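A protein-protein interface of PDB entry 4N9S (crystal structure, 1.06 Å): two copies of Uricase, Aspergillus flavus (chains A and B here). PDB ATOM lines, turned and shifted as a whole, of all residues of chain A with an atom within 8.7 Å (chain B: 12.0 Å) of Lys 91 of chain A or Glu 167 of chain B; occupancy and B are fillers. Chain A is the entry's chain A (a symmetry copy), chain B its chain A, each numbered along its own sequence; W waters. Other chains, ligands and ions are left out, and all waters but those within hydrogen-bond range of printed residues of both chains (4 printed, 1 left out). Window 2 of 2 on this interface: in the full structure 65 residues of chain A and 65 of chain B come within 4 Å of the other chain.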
ATOM      1  N   VAL A  56       4.747 -26.691   8.466  1.00  0.00           N
ATOM      2  CA  VAL A  56       5.661 -25.984   7.585  1.00  0.00           C
ATOM      3  C   VAL A  56       4.869 -24.742   7.130  1.00  0.00           C
ATOM      4  O   VAL A  56       3.853 -24.870   6.447  1.00  0.00           O
ATOM      5  CB  VAL A  56       6.084 -26.870   6.386  1.00  0.00           C
ATOM      6  CG1 VAL A  56       6.963 -26.098   5.428  1.00  0.00           C
ATOM      7  CG2 VAL A  56       6.793 -28.150   6.877  1.00  0.00           C
ATOM      8  N   SER A  60       6.700 -20.237   4.243  1.00  0.00           N
ATOM      9  CA  SER A  60       7.890 -21.019   3.918  1.00  0.00           C
ATOM     10  C   SER A  60       7.703 -21.857   2.660  1.00  0.00           C
ATOM     11  O   SER A  60       8.641 -22.040   1.889  1.00  0.00           O
ATOM     12  CB  SER A  60       8.273 -21.933   5.079  1.00  0.00           C
ATOM     13  OG  SER A  60       8.436 -21.168   6.253  1.00  0.00           O
ATOM     14  N   ASN A  63       8.377 -19.417  -0.048  1.00  0.00           N
ATOM     15  CA  ASN A  63       9.819 -19.247  -0.231  1.00  0.00           C
ATOM     16  C   ASN A  63      10.413 -20.413  -1.012  1.00  0.00           C
ATOM     17  O   ASN A  63      11.272 -20.234  -1.865  1.00  0.00           O
ATOM     18  CB  ASN A  63      10.548 -19.157   1.115  1.00  0.00           C
ATOM     19  CG  ASN A  63      10.230 -17.882   1.885  1.00  0.00           C
ATOM     20  OD1 ASN A  63       9.822 -16.858   1.306  1.00  0.00           O
ATOM     21  ND2 ASN A  63      10.442 -17.924   3.198  1.00  0.00           N
ATOM     22  N   THR A  64       9.981 -21.619  -0.650  1.00  0.00           N
ATOM     23  CA  THR A  64      10.500 -22.837  -1.247  1.00  0.00           C
ATOM     24  C   THR A  64      10.158 -22.909  -2.732  1.00  0.00           C
ATOM     25  O   THR A  64      10.969 -23.390  -3.522  1.00  0.00           O
ATOM     26  CB  THR A  64       9.974 -24.076  -0.494  1.00  0.00           C
ATOM     27  OG1 THR A  64      10.338 -23.995   0.890  1.00  0.00           O
ATOM     28  CG2 THR A  64      10.511 -25.362  -1.069  1.00  0.00           C
ATOM     29  N   ILE A  67      12.758 -20.618  -4.389  1.00  0.00           N
ATOM     30  CA  ILE A  67      14.083 -21.233  -4.310  1.00  0.00           C
ATOM     31  C   ILE A  67      14.195 -22.388  -5.299  1.00  0.00           C
ATOM     32  O   ILE A  67      15.197 -22.538  -6.003  1.00  0.00           O
ATOM     33  CB  ILE A  67      14.369 -21.693  -2.869  1.00  0.00           C
ATOM     34  CG1 ILE A  67      14.572 -20.480  -1.957  1.00  0.00           C
ATOM     35  CG2 ILE A  67      15.572 -22.630  -2.827  1.00  0.00           C
ATOM     36  CD1 ILE A  67      14.394 -20.789  -0.478  1.00  0.00           C
ATOM     37  N   LEU A  84       9.325 -30.115  -7.132  1.00  0.00           N
ATOM     38  CA  LEU A  84       8.810 -29.362  -6.009  1.00  0.00           C
ATOM     39  C   LEU A  84       8.090 -30.272  -5.007  1.00  0.00           C
ATOM     40  O   LEU A  84       8.312 -30.196  -3.798  1.00  0.00           O
ATOM     41  CB  LEU A  84       7.869 -28.297  -6.547  1.00  0.00           C
ATOM     42  CG  LEU A  84       7.330 -27.231  -5.625  1.00  0.00           C
ATOM     43  CD1 LEU A  84       8.414 -26.480  -4.879  1.00  0.00           C
ATOM     44  CD2 LEU A  84       6.495 -26.269  -6.484  1.00  0.00           C
ATOM     45  N   GLY A  85       7.210 -31.144  -5.496  1.00  0.00           N
ATOM     46  CA  GLY A  85       6.486 -32.025  -4.602  1.00  0.00           C
ATOM     47  C   GLY A  85       7.395 -33.032  -3.897  1.00  0.00           C
ATOM     48  O   GLY A  85       7.215 -33.315  -2.713  1.00  0.00           O
ATOM     49  N   THR A  86       8.376 -33.567  -4.623  1.00  0.00           N
ATOM     50  CA  THR A  86       9.343 -34.492  -4.052  1.00  0.00           C
ATOM     51  C   THR A  86      10.118 -33.825  -2.920  1.00  0.00           C
ATOM     52  O   THR A  86      10.386 -34.454  -1.894  1.00  0.00           O
ATOM     53  CB  THR A  86      10.278 -35.026  -5.145  1.00  0.00           C
ATOM     54  OG1 THR A  86       9.515 -35.810  -6.067  1.00  0.00           O
ATOM     55  CG2 THR A  86      11.367 -35.913  -4.551  1.00  0.00           C
ATOM     56  N   HIS A  87      10.477 -32.555  -3.094  1.00  0.00           N
ATOM     57  CA  HIS A  87      11.187 -31.840  -2.058  1.00  0.00           C
ATOM     58  C   HIS A  87      10.442 -31.904  -0.728  1.00  0.00           C
ATOM     59  O   HIS A  87      11.046 -32.203   0.303  1.00  0.00           O
ATOM     60  CB  HIS A  87      11.413 -30.375  -2.439  1.00  0.00           C
ATOM     61  CG  HIS A  87      11.784 -29.540  -1.262  1.00  0.00           C
ATOM     62  ND1 HIS A  87      13.052 -29.540  -0.714  1.00  0.00           N
ATOM     63  CD2 HIS A  87      11.022 -28.769  -0.457  1.00  0.00           C
ATOM     64  CE1 HIS A  87      13.058 -28.763   0.351  1.00  0.00           C
ATOM     65  NE2 HIS A  87      11.842 -28.277   0.525  1.00  0.00           N
ATOM     66  N   PHE A  88       9.140 -31.615  -0.729  1.00  0.00           N
ATOM     67  CA  PHE A  88       8.429 -31.526   0.538  1.00  0.00           C
ATOM     68  C   PHE A  88       8.339 -32.880   1.249  1.00  0.00           C
ATOM     69  O   PHE A  88       8.496 -32.950   2.466  1.00  0.00           O
ATOM     70  CB  PHE A  88       7.040 -30.917   0.364  1.00  0.00           C
ATOM     71  CG  PHE A  88       7.088 -29.451   0.060  1.00  0.00           C
ATOM     72  CD1 PHE A  88       7.402 -28.535   1.046  1.00  0.00           C
ATOM     73  CD2 PHE A  88       6.873 -28.984  -1.224  1.00  0.00           C
ATOM     74  CE1 PHE A  88       7.478 -27.178   0.763  1.00  0.00           C
ATOM     75  CE2 PHE A  88       6.947 -27.626  -1.508  1.00  0.00           C
ATOM     76  CZ  PHE A  88       7.244 -26.728  -0.514  1.00  0.00           C
ATOM     77  N   ILE A  89       8.057 -33.953   0.513  1.00  0.00           N
ATOM     78  CA  ILE A  89       7.949 -35.250   1.173  1.00  0.00           C
ATOM     79  C   ILE A  89       9.314 -35.802   1.600  1.00  0.00           C
ATOM     80  O   ILE A  89       9.384 -36.574   2.534  1.00  0.00           O
ATOM     81  CB  ILE A  89       7.154 -36.304   0.354  1.00  0.00           C
ATOM     82  CG1 ILE A  89       7.864 -36.698  -0.939  1.00  0.00           C
ATOM     83  CG2 ILE A  89       5.732 -35.813   0.099  1.00  0.00           C
ATOM     84  CD1 ILE A  89       7.437 -38.081  -1.460  1.00  0.00           C
ATOM     85  N   GLU A  90      10.401 -35.402   0.951  1.00  0.00           N
ATOM     86  CA  GLU A  90      11.732 -35.857   1.355  1.00  0.00           C
ATOM     87  C   GLU A  90      12.281 -35.022   2.504  1.00  0.00           C
ATOM     88  O   GLU A  90      12.916 -35.541   3.413  1.00  0.00           O
ATOM     89  CB  GLU A  90      12.693 -35.850   0.161  1.00  0.00           C
ATOM     90  CG  GLU A  90      12.393 -36.943  -0.844  1.00  0.00           C
ATOM     91  CD  GLU A  90      13.410 -37.055  -1.966  1.00  0.00           C
ATOM     92  OE1 GLU A  90      14.242 -36.137  -2.135  1.00  0.00           O
ATOM     93  OE2 GLU A  90      13.350 -38.062  -2.699  1.00  0.00           O
ATOM     94  N   LYS A  91      12.055 -33.718   2.463  1.00  0.00           N
ATOM     95  CA  LYS A  91      12.632 -32.820   3.453  1.00  0.00           C
ATOM     96  C   LYS A  91      11.998 -32.988   4.832  1.00  0.00           C
ATOM     97  O   LYS A  91      12.684 -32.884   5.854  1.00  0.00           O
ATOM     98  CB  LYS A  91      12.521 -31.361   2.983  1.00  0.00           C
ATOM     99  CG  LYS A  91      13.053 -30.336   3.968  1.00  0.00           C
ATOM    100  CD  LYS A  91      14.560 -30.443   4.115  1.00  0.00           C
ATOM    101  CE  LYS A  91      15.076 -29.508   5.189  1.00  0.00           C
ATOM    102  NZ  LYS A  91      16.558 -29.580   5.277  1.00  0.00           N
ATOM    103  N   TYR A  92      10.690 -33.242   4.855  1.00  0.00           N
ATOM    104  CA  TYR A  92       9.927 -33.282   6.093  1.00  0.00           C
ATOM    105  C   TYR A  92       9.422 -34.701   6.333  1.00  0.00           C
ATOM    106  O   TYR A  92       8.576 -35.199   5.608  1.00  0.00           O
ATOM    107  CB  TYR A  92       8.763 -32.276   6.049  1.00  0.00           C
ATOM    108  CG  TYR A  92       9.285 -30.880   5.825  1.00  0.00           C
ATOM    109  CD1 TYR A  92       9.953 -30.206   6.831  1.00  0.00           C
ATOM    110  CD2 TYR A  92       9.158 -30.252   4.592  1.00  0.00           C
ATOM    111  CE1 TYR A  92      10.496 -28.943   6.629  1.00  0.00           C
ATOM    112  CE2 TYR A  92       9.671 -28.983   4.378  1.00  0.00           C
ATOM    113  CZ  TYR A  92      10.350 -28.335   5.404  1.00  0.00           C
ATOM    114  OH  TYR A  92      10.876 -27.081   5.189  1.00  0.00           O
ATOM    115  N   ASN A  93       9.954 -35.362   7.351  1.00  0.00           N
ATOM    116  CA  ASN A  93       9.576 -36.741   7.623  1.00  0.00           C
ATOM    117  C   ASN A  93       8.056 -36.911   7.715  1.00  0.00           C
ATOM    118  O   ASN A  93       7.485 -37.861   7.163  1.00  0.00           O
ATOM    119  CB  ASN A  93      10.247 -37.225   8.912  1.00  0.00           C
ATOM    120  CG  ASN A  93      11.730 -37.443   8.746  1.00  0.00           C
ATOM    121  OD1 ASN A  93      12.259 -37.411   7.634  1.00  0.00           O
ATOM    122  ND2 ASN A  93      12.413 -37.679   9.854  1.00  0.00           N
ATOM    123  N   HIS A  94       7.394 -35.975   8.385  1.00  0.00           N
ATOM    124  CA  HIS A  94       5.978 -36.115   8.697  1.00  0.00           C
ATOM    125  C   HIS A  94       5.030 -35.658   7.597  1.00  0.00           C
ATOM    126  O   HIS A  94       3.826 -35.806   7.729  1.00  0.00           O
ATOM    127  CB  HIS A  94       5.657 -35.370   9.989  1.00  0.00           C
ATOM    128  CG  HIS A  94       5.653 -33.886   9.845  1.00  0.00           C
ATOM    129  ND1 HIS A  94       6.798 -33.149   9.630  1.00  0.00           N
ATOM    130  CD2 HIS A  94       4.634 -32.998   9.895  1.00  0.00           C
ATOM    131  CE1 HIS A  94       6.481 -31.872   9.534  1.00  0.00           C
ATOM    132  NE2 HIS A  94       5.178 -31.754   9.700  1.00  0.00           N
ATOM    133  N   ILE A  95       5.572 -35.088   6.529  1.00  0.00           N
ATOM    134  CA  ILE A  95       4.765 -34.717   5.372  1.00  0.00           C
ATOM    135  C   ILE A  95       4.799 -35.878   4.396  1.00  0.00           C
ATOM    136  O   ILE A  95       5.867 -36.331   4.021  1.00  0.00           O
ATOM    137  CB  ILE A  95       5.320 -33.444   4.700  1.00  0.00           C
ATOM    138  CG1 ILE A  95       5.224 -32.258   5.661  1.00  0.00           C
ATOM    139  CG2 ILE A  95       4.584 -33.163   3.399  1.00  0.00           C
ATOM    140  CD1 ILE A  95       3.812 -31.912   6.124  1.00  0.00           C
ATOM    141  N   GLU A 137       4.211 -40.161  -0.718  1.00  0.00           N
ATOM    142  CA  GLU A 137       5.329 -40.930  -0.206  1.00  0.00           C
ATOM    143  C   GLU A 137       5.004 -42.414  -0.261  1.00  0.00           C
ATOM    144  O   GLU A 137       3.956 -42.856   0.219  1.00  0.00           O
ATOM    145  CB  GLU A 137       5.657 -40.473   1.216  1.00  0.00           C
ATOM    146  CG  GLU A 137       6.996 -40.995   1.708  1.00  0.00           C
ATOM    147  CD  GLU A 137       7.444 -40.384   3.013  1.00  0.00           C
ATOM    148  OE1 GLU A 137       6.898 -39.360   3.454  1.00  0.00           O
ATOM    149  OE2 GLU A 137       8.386 -40.924   3.617  1.00  0.00           O
ATOM    150  N   PHE B 163       5.404 -22.521  14.838  1.00  0.00           N
ATOM    151  CA  PHE B 163       5.502 -23.302  13.625  1.00  0.00           C
ATOM    152  C   PHE B 163       6.945 -23.730  13.363  1.00  0.00           C
ATOM    153  O   PHE B 163       7.897 -23.206  13.957  1.00  0.00           O
ATOM    154  CB  PHE B 163       4.909 -22.525  12.442  1.00  0.00           C
ATOM    155  CG  PHE B 163       5.451 -21.128  12.291  1.00  0.00           C
ATOM    156  CD1 PHE B 163       4.809 -20.060  12.899  1.00  0.00           C
ATOM    157  CD2 PHE B 163       6.588 -20.883  11.549  1.00  0.00           C
ATOM    158  CE1 PHE B 163       5.277 -18.764  12.759  1.00  0.00           C
ATOM    159  CE2 PHE B 163       7.063 -19.594  11.399  1.00  0.00           C
ATOM    160  CZ  PHE B 163       6.407 -18.537  12.016  1.00  0.00           C
ATOM    161  N   LEU B 164       7.103 -24.703  12.478  1.00  0.00           N
ATOM    162  CA  LEU B 164       8.415 -25.243  12.153  1.00  0.00           C
ATOM    163  C   LEU B 164       9.305 -24.151  11.567  1.00  0.00           C
ATOM    164  O   LEU B 164       8.875 -23.375  10.709  1.00  0.00           O
ATOM    165  CB  LEU B 164       8.249 -26.417  11.184  1.00  0.00           C
ATOM    166  CG  LEU B 164       9.499 -27.207  10.807  1.00  0.00           C
ATOM    167  CD1 LEU B 164       9.129 -28.638  10.458  1.00  0.00           C
ATOM    168  CD2 LEU B 164      10.240 -26.557   9.651  1.00  0.00           C
ATOM    169  N   ARG B 165      10.546 -24.098  12.040  1.00  0.00           N
ATOM    170  CA  ARG B 165      11.514 -23.121  11.567  1.00  0.00           C
ATOM    171  C   ARG B 165      12.762 -23.844  11.080  1.00  0.00           C
ATOM    172  O   ARG B 165      13.418 -24.561  11.845  1.00  0.00           O
ATOM    173  CB  ARG B 165      11.892 -22.132  12.678  1.00  0.00           C
ATOM    174  CG  ARG B 165      10.739 -21.452  13.412  1.00  0.00           C
ATOM    175  CD  ARG B 165      11.236 -20.238  14.228  1.00  0.00           C
ATOM    176  NE  ARG B 165      11.698 -19.189  13.328  1.00  0.00           N
ATOM    177  CZ  ARG B 165      10.894 -18.291  12.767  1.00  0.00           C
ATOM    178  NH1 ARG B 165       9.607 -18.300  13.059  1.00  0.00           N
ATOM    179  NH2 ARG B 165      11.355 -17.382  11.923  1.00  0.00           N
ATOM    180  N   ASP B 166      13.094 -23.656   9.809  1.00  0.00           N
ATOM    181  CA  ASP B 166      14.302 -24.214   9.233  1.00  0.00           C
ATOM    182  C   ASP B 166      14.883 -23.236   8.219  1.00  0.00           C
ATOM    183  O   ASP B 166      14.543 -22.040   8.213  1.00  0.00           O
ATOM    184  CB  ASP B 166      14.051 -25.614   8.643  1.00  0.00           C
ATOM    185  CG  ASP B 166      13.133 -25.609   7.431  1.00  0.00           C
ATOM    186  OD1 ASP B 166      12.768 -24.515   6.925  1.00  0.00           O
ATOM    187  OD2 ASP B 166      12.786 -26.730   6.984  1.00  0.00           O
ATOM    188  N   GLU B 167      15.761 -23.719   7.353  1.00  0.00           N
ATOM    189  CA  GLU B 167      16.464 -22.844   6.437  1.00  0.00           C
ATOM    190  C   GLU B 167      15.582 -22.268   5.318  1.00  0.00           C
ATOM    191  O   GLU B 167      16.073 -21.445   4.548  1.00  0.00           O
ATOM    192  CB  GLU B 167      17.696 -23.555   5.851  1.00  0.00           C
ATOM    193  CG  GLU B 167      17.414 -24.726   4.908  1.00  0.00           C
ATOM    194  CD  GLU B 167      17.240 -26.089   5.589  1.00  0.00           C
ATOM    195  OE1 GLU B 167      16.898 -26.165   6.788  1.00  0.00           O
ATOM    196  OE2 GLU B 167      17.445 -27.108   4.896  1.00  0.00           O
ATOM    197  N   TYR B 168      14.315 -22.678   5.234  1.00  0.00           N
ATOM    198  CA  TYR B 168      13.367 -22.109   4.278  1.00  0.00           C
ATOM    199  C   TYR B 168      12.455 -21.073   4.927  1.00  0.00           C
ATOM    200  O   TYR B 168      11.593 -20.492   4.253  1.00  0.00           O
ATOM    201  CB  TYR B 168      12.510 -23.235   3.678  1.00  0.00           C
ATOM    202  CG  TYR B 168      13.324 -24.218   2.897  1.00  0.00           C
ATOM    203  CD1 TYR B 168      13.599 -24.020   1.553  1.00  0.00           C
ATOM    204  CD2 TYR B 168      13.855 -25.335   3.516  1.00  0.00           C
ATOM    205  CE1 TYR B 168      14.370 -24.911   0.844  1.00  0.00           C
ATOM    206  CE2 TYR B 168      14.623 -26.223   2.827  1.00  0.00           C
ATOM    207  CZ  TYR B 168      14.883 -26.020   1.495  1.00  0.00           C
ATOM    208  OH  TYR B 168      15.666 -26.935   0.831  1.00  0.00           O
ATOM    209  N   THR B 169      12.639 -20.828   6.223  1.00  0.00           N
ATOM    210  CA  THR B 169      11.705 -20.018   7.005  1.00  0.00           C
ATOM    211  C   THR B 169      12.194 -18.593   7.223  1.00  0.00           C
ATOM    212  O   THR B 169      13.292 -18.397   7.737  1.00  0.00           O
ATOM    213  CB  THR B 169      11.474 -20.647   8.399  1.00  0.00           C
ATOM    214  OG1 THR B 169      11.165 -22.037   8.272  1.00  0.00           O
ATOM    215  CG2 THR B 169      10.371 -19.937   9.156  1.00  0.00           C
ATOM    216  N   THR B 170      11.372 -17.616   6.850  1.00  0.00           N
ATOM    217  CA  THR B 170      11.602 -16.221   7.155  1.00  0.00           C
ATOM    218  C   THR B 170      10.491 -15.611   8.008  1.00  0.00           C
ATOM    219  O   THR B 170      10.665 -14.556   8.609  1.00  0.00           O
ATOM    220  CB  THR B 170      11.744 -15.387   5.871  1.00  0.00           C
ATOM    221  OG1 THR B 170      10.583 -15.577   5.051  1.00  0.00           O
ATOM    222  CG2 THR B 170      12.956 -15.799   5.084  1.00  0.00           C
ATOM    223  N   LEU B 171       9.332 -16.254   8.046  1.00  0.00           N
ATOM    224  CA  LEU B 171       8.180 -15.681   8.733  1.00  0.00           C
ATOM    225  C   LEU B 171       8.431 -15.475  10.216  1.00  0.00           C
ATOM    226  O   LEU B 171       8.840 -16.391  10.913  1.00  0.00           O
ATOM    227  CB  LEU B 171       6.962 -16.598   8.557  1.00  0.00           C
ATOM    228  CG  LEU B 171       5.638 -16.133   9.171  1.00  0.00           C
ATOM    229  CD1 LEU B 171       5.102 -14.869   8.490  1.00  0.00           C
ATOM    230  CD2 LEU B 171       4.600 -17.237   9.092  1.00  0.00           C
HETATM  231  O   HOH W   1      10.050 -24.503   6.410  1.00  0.00           O
HETATM  232  O   HOH W   2       8.563 -14.885   2.701  1.00  0.00           O
HETATM  233  O   HOH W   3      16.567 -28.566   8.079  1.00  0.00           O
HETATM  234  O   HOH W   4       8.261 -23.258   8.064  1.00  0.00           O
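Of the 9 printed residues of chain B, 6 touch a printed residue of chain A.
Hydrophobic or aromatic side chains of chain A within 4 Å of the printed part of chain B: Ile 67, His 87 and Tyr 92.
Among the printed residues, 11 pairs touch across the chains.
Among the printed residues, Asp or Glu carboxylates within 4 Å of a Lys or Arg side-chain nitrogen of the other chain: Lys 91 of chain A with Glu 167 of chain B (2.7 Å).
OD1 of Asp 166 of chain B lies within hydrogen-bond range of N of Tyr 168 of chain B.
The side-chain hydroxyl (OG1) of Thr 169 of chain B sits at hydrogen-bond distance from the backbone NH (N) of Asp 166 of chain B.
OG1 of Thr 64 of chain A lies within hydrogen-bond range of O of Ser 60 of chain A.
Water W4 lies within hydrogen-bond range of O of Leu 164 of chain B (2.7 Å), OG of Ser 60 of chain A (2.8 Å) and OG1 of Thr 169 of chain B (3.2 Å).
Water W2 bridges OD1 of Asn 63 of chain A and OG1 of Thr 170 of chain B.
Water W3 lies within hydrogen-bond range of OE1 of Glu 167 of chain B and NZ of Lys 91 of chain A.
Water W1 lies within hydrogen-bond range of OD1 of Asp 166 of chain B, OH of Tyr 92 of chain A and OG1 of Thr 169 of chain B.
Lys 91 of chain A touches just one residue of chain B: Glu 167 (2.7 Å).
Glu 167 of chain B touches just one residue of chain A: Lys 91.
His 87 of chain A touches just one residue of chain B: Tyr 168 (3.2 Å).
No residue of chain B comes within 4 Å of Ile 89 of chain A.
Tyr 92 of chain A touches just these residues of chain B: Leu 164, Asp 166 and Tyr 168.
No residue of chain B comes within 4 Å of Asn 93 of chain A.
Of the printed residues of chain A, Asp 166 of chain B touches Tyr 92 (2.6 Å).
Of the printed residues of chain B, Asn 63 of chain A touches Tyr 168 and Thr 170.
Of the printed residues of chain A, Thr 170 of chain B touches Asn 63.
Of the printed residues of chain A, Thr 169 of chain B touches Ser 60.
Thr 86 of chain A touches none of the printed residues of chain B.
No position is printed for both chains.
O of Tyr 168 of chain B touches CB of Ser 60 of chain A, at 3.7 Å.
Thr 169 of chain B touches Ser 60 of chain A.
OG1 of Thr 64 of chain A touches CD1 of Tyr 168 of chain B, 3.3 Å away.
Ile 67 of chain A touches Tyr 168 of chain B (CD1 to CD1, 3.9 Å).
Tyr 168 of chain B touches His 87 of chain A (OH to CE1, 3.2 Å).
Tyr 92 of chain A touches Leu 164 of chain B (CE1 to CD2, 3.9 Å).
OH of Tyr 92 of chain A touches CD2 of Tyr 168 of chain B, 3.8 Å away.
The side-chain carboxylate (OD2) of Asp 166 of chain B is in hydrogen-bond range of the side-chain hydroxyl (OH) of Tyr 92 of chain A (2.6 Å).
NZ of Lys 91 of chain A is in salt-bridge range of OE2 of Glu 167 of chain B (2.7 Å).
O of Tyr 168 of chain B sits at hydrogen-bond distance from ND2 of Asn 63 of chain A, 3.0 Å away.
ND2 of Asn 63 of chain A sits at hydrogen-bond distance from OG1 of Thr 170 of chain B (3.0 Å).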
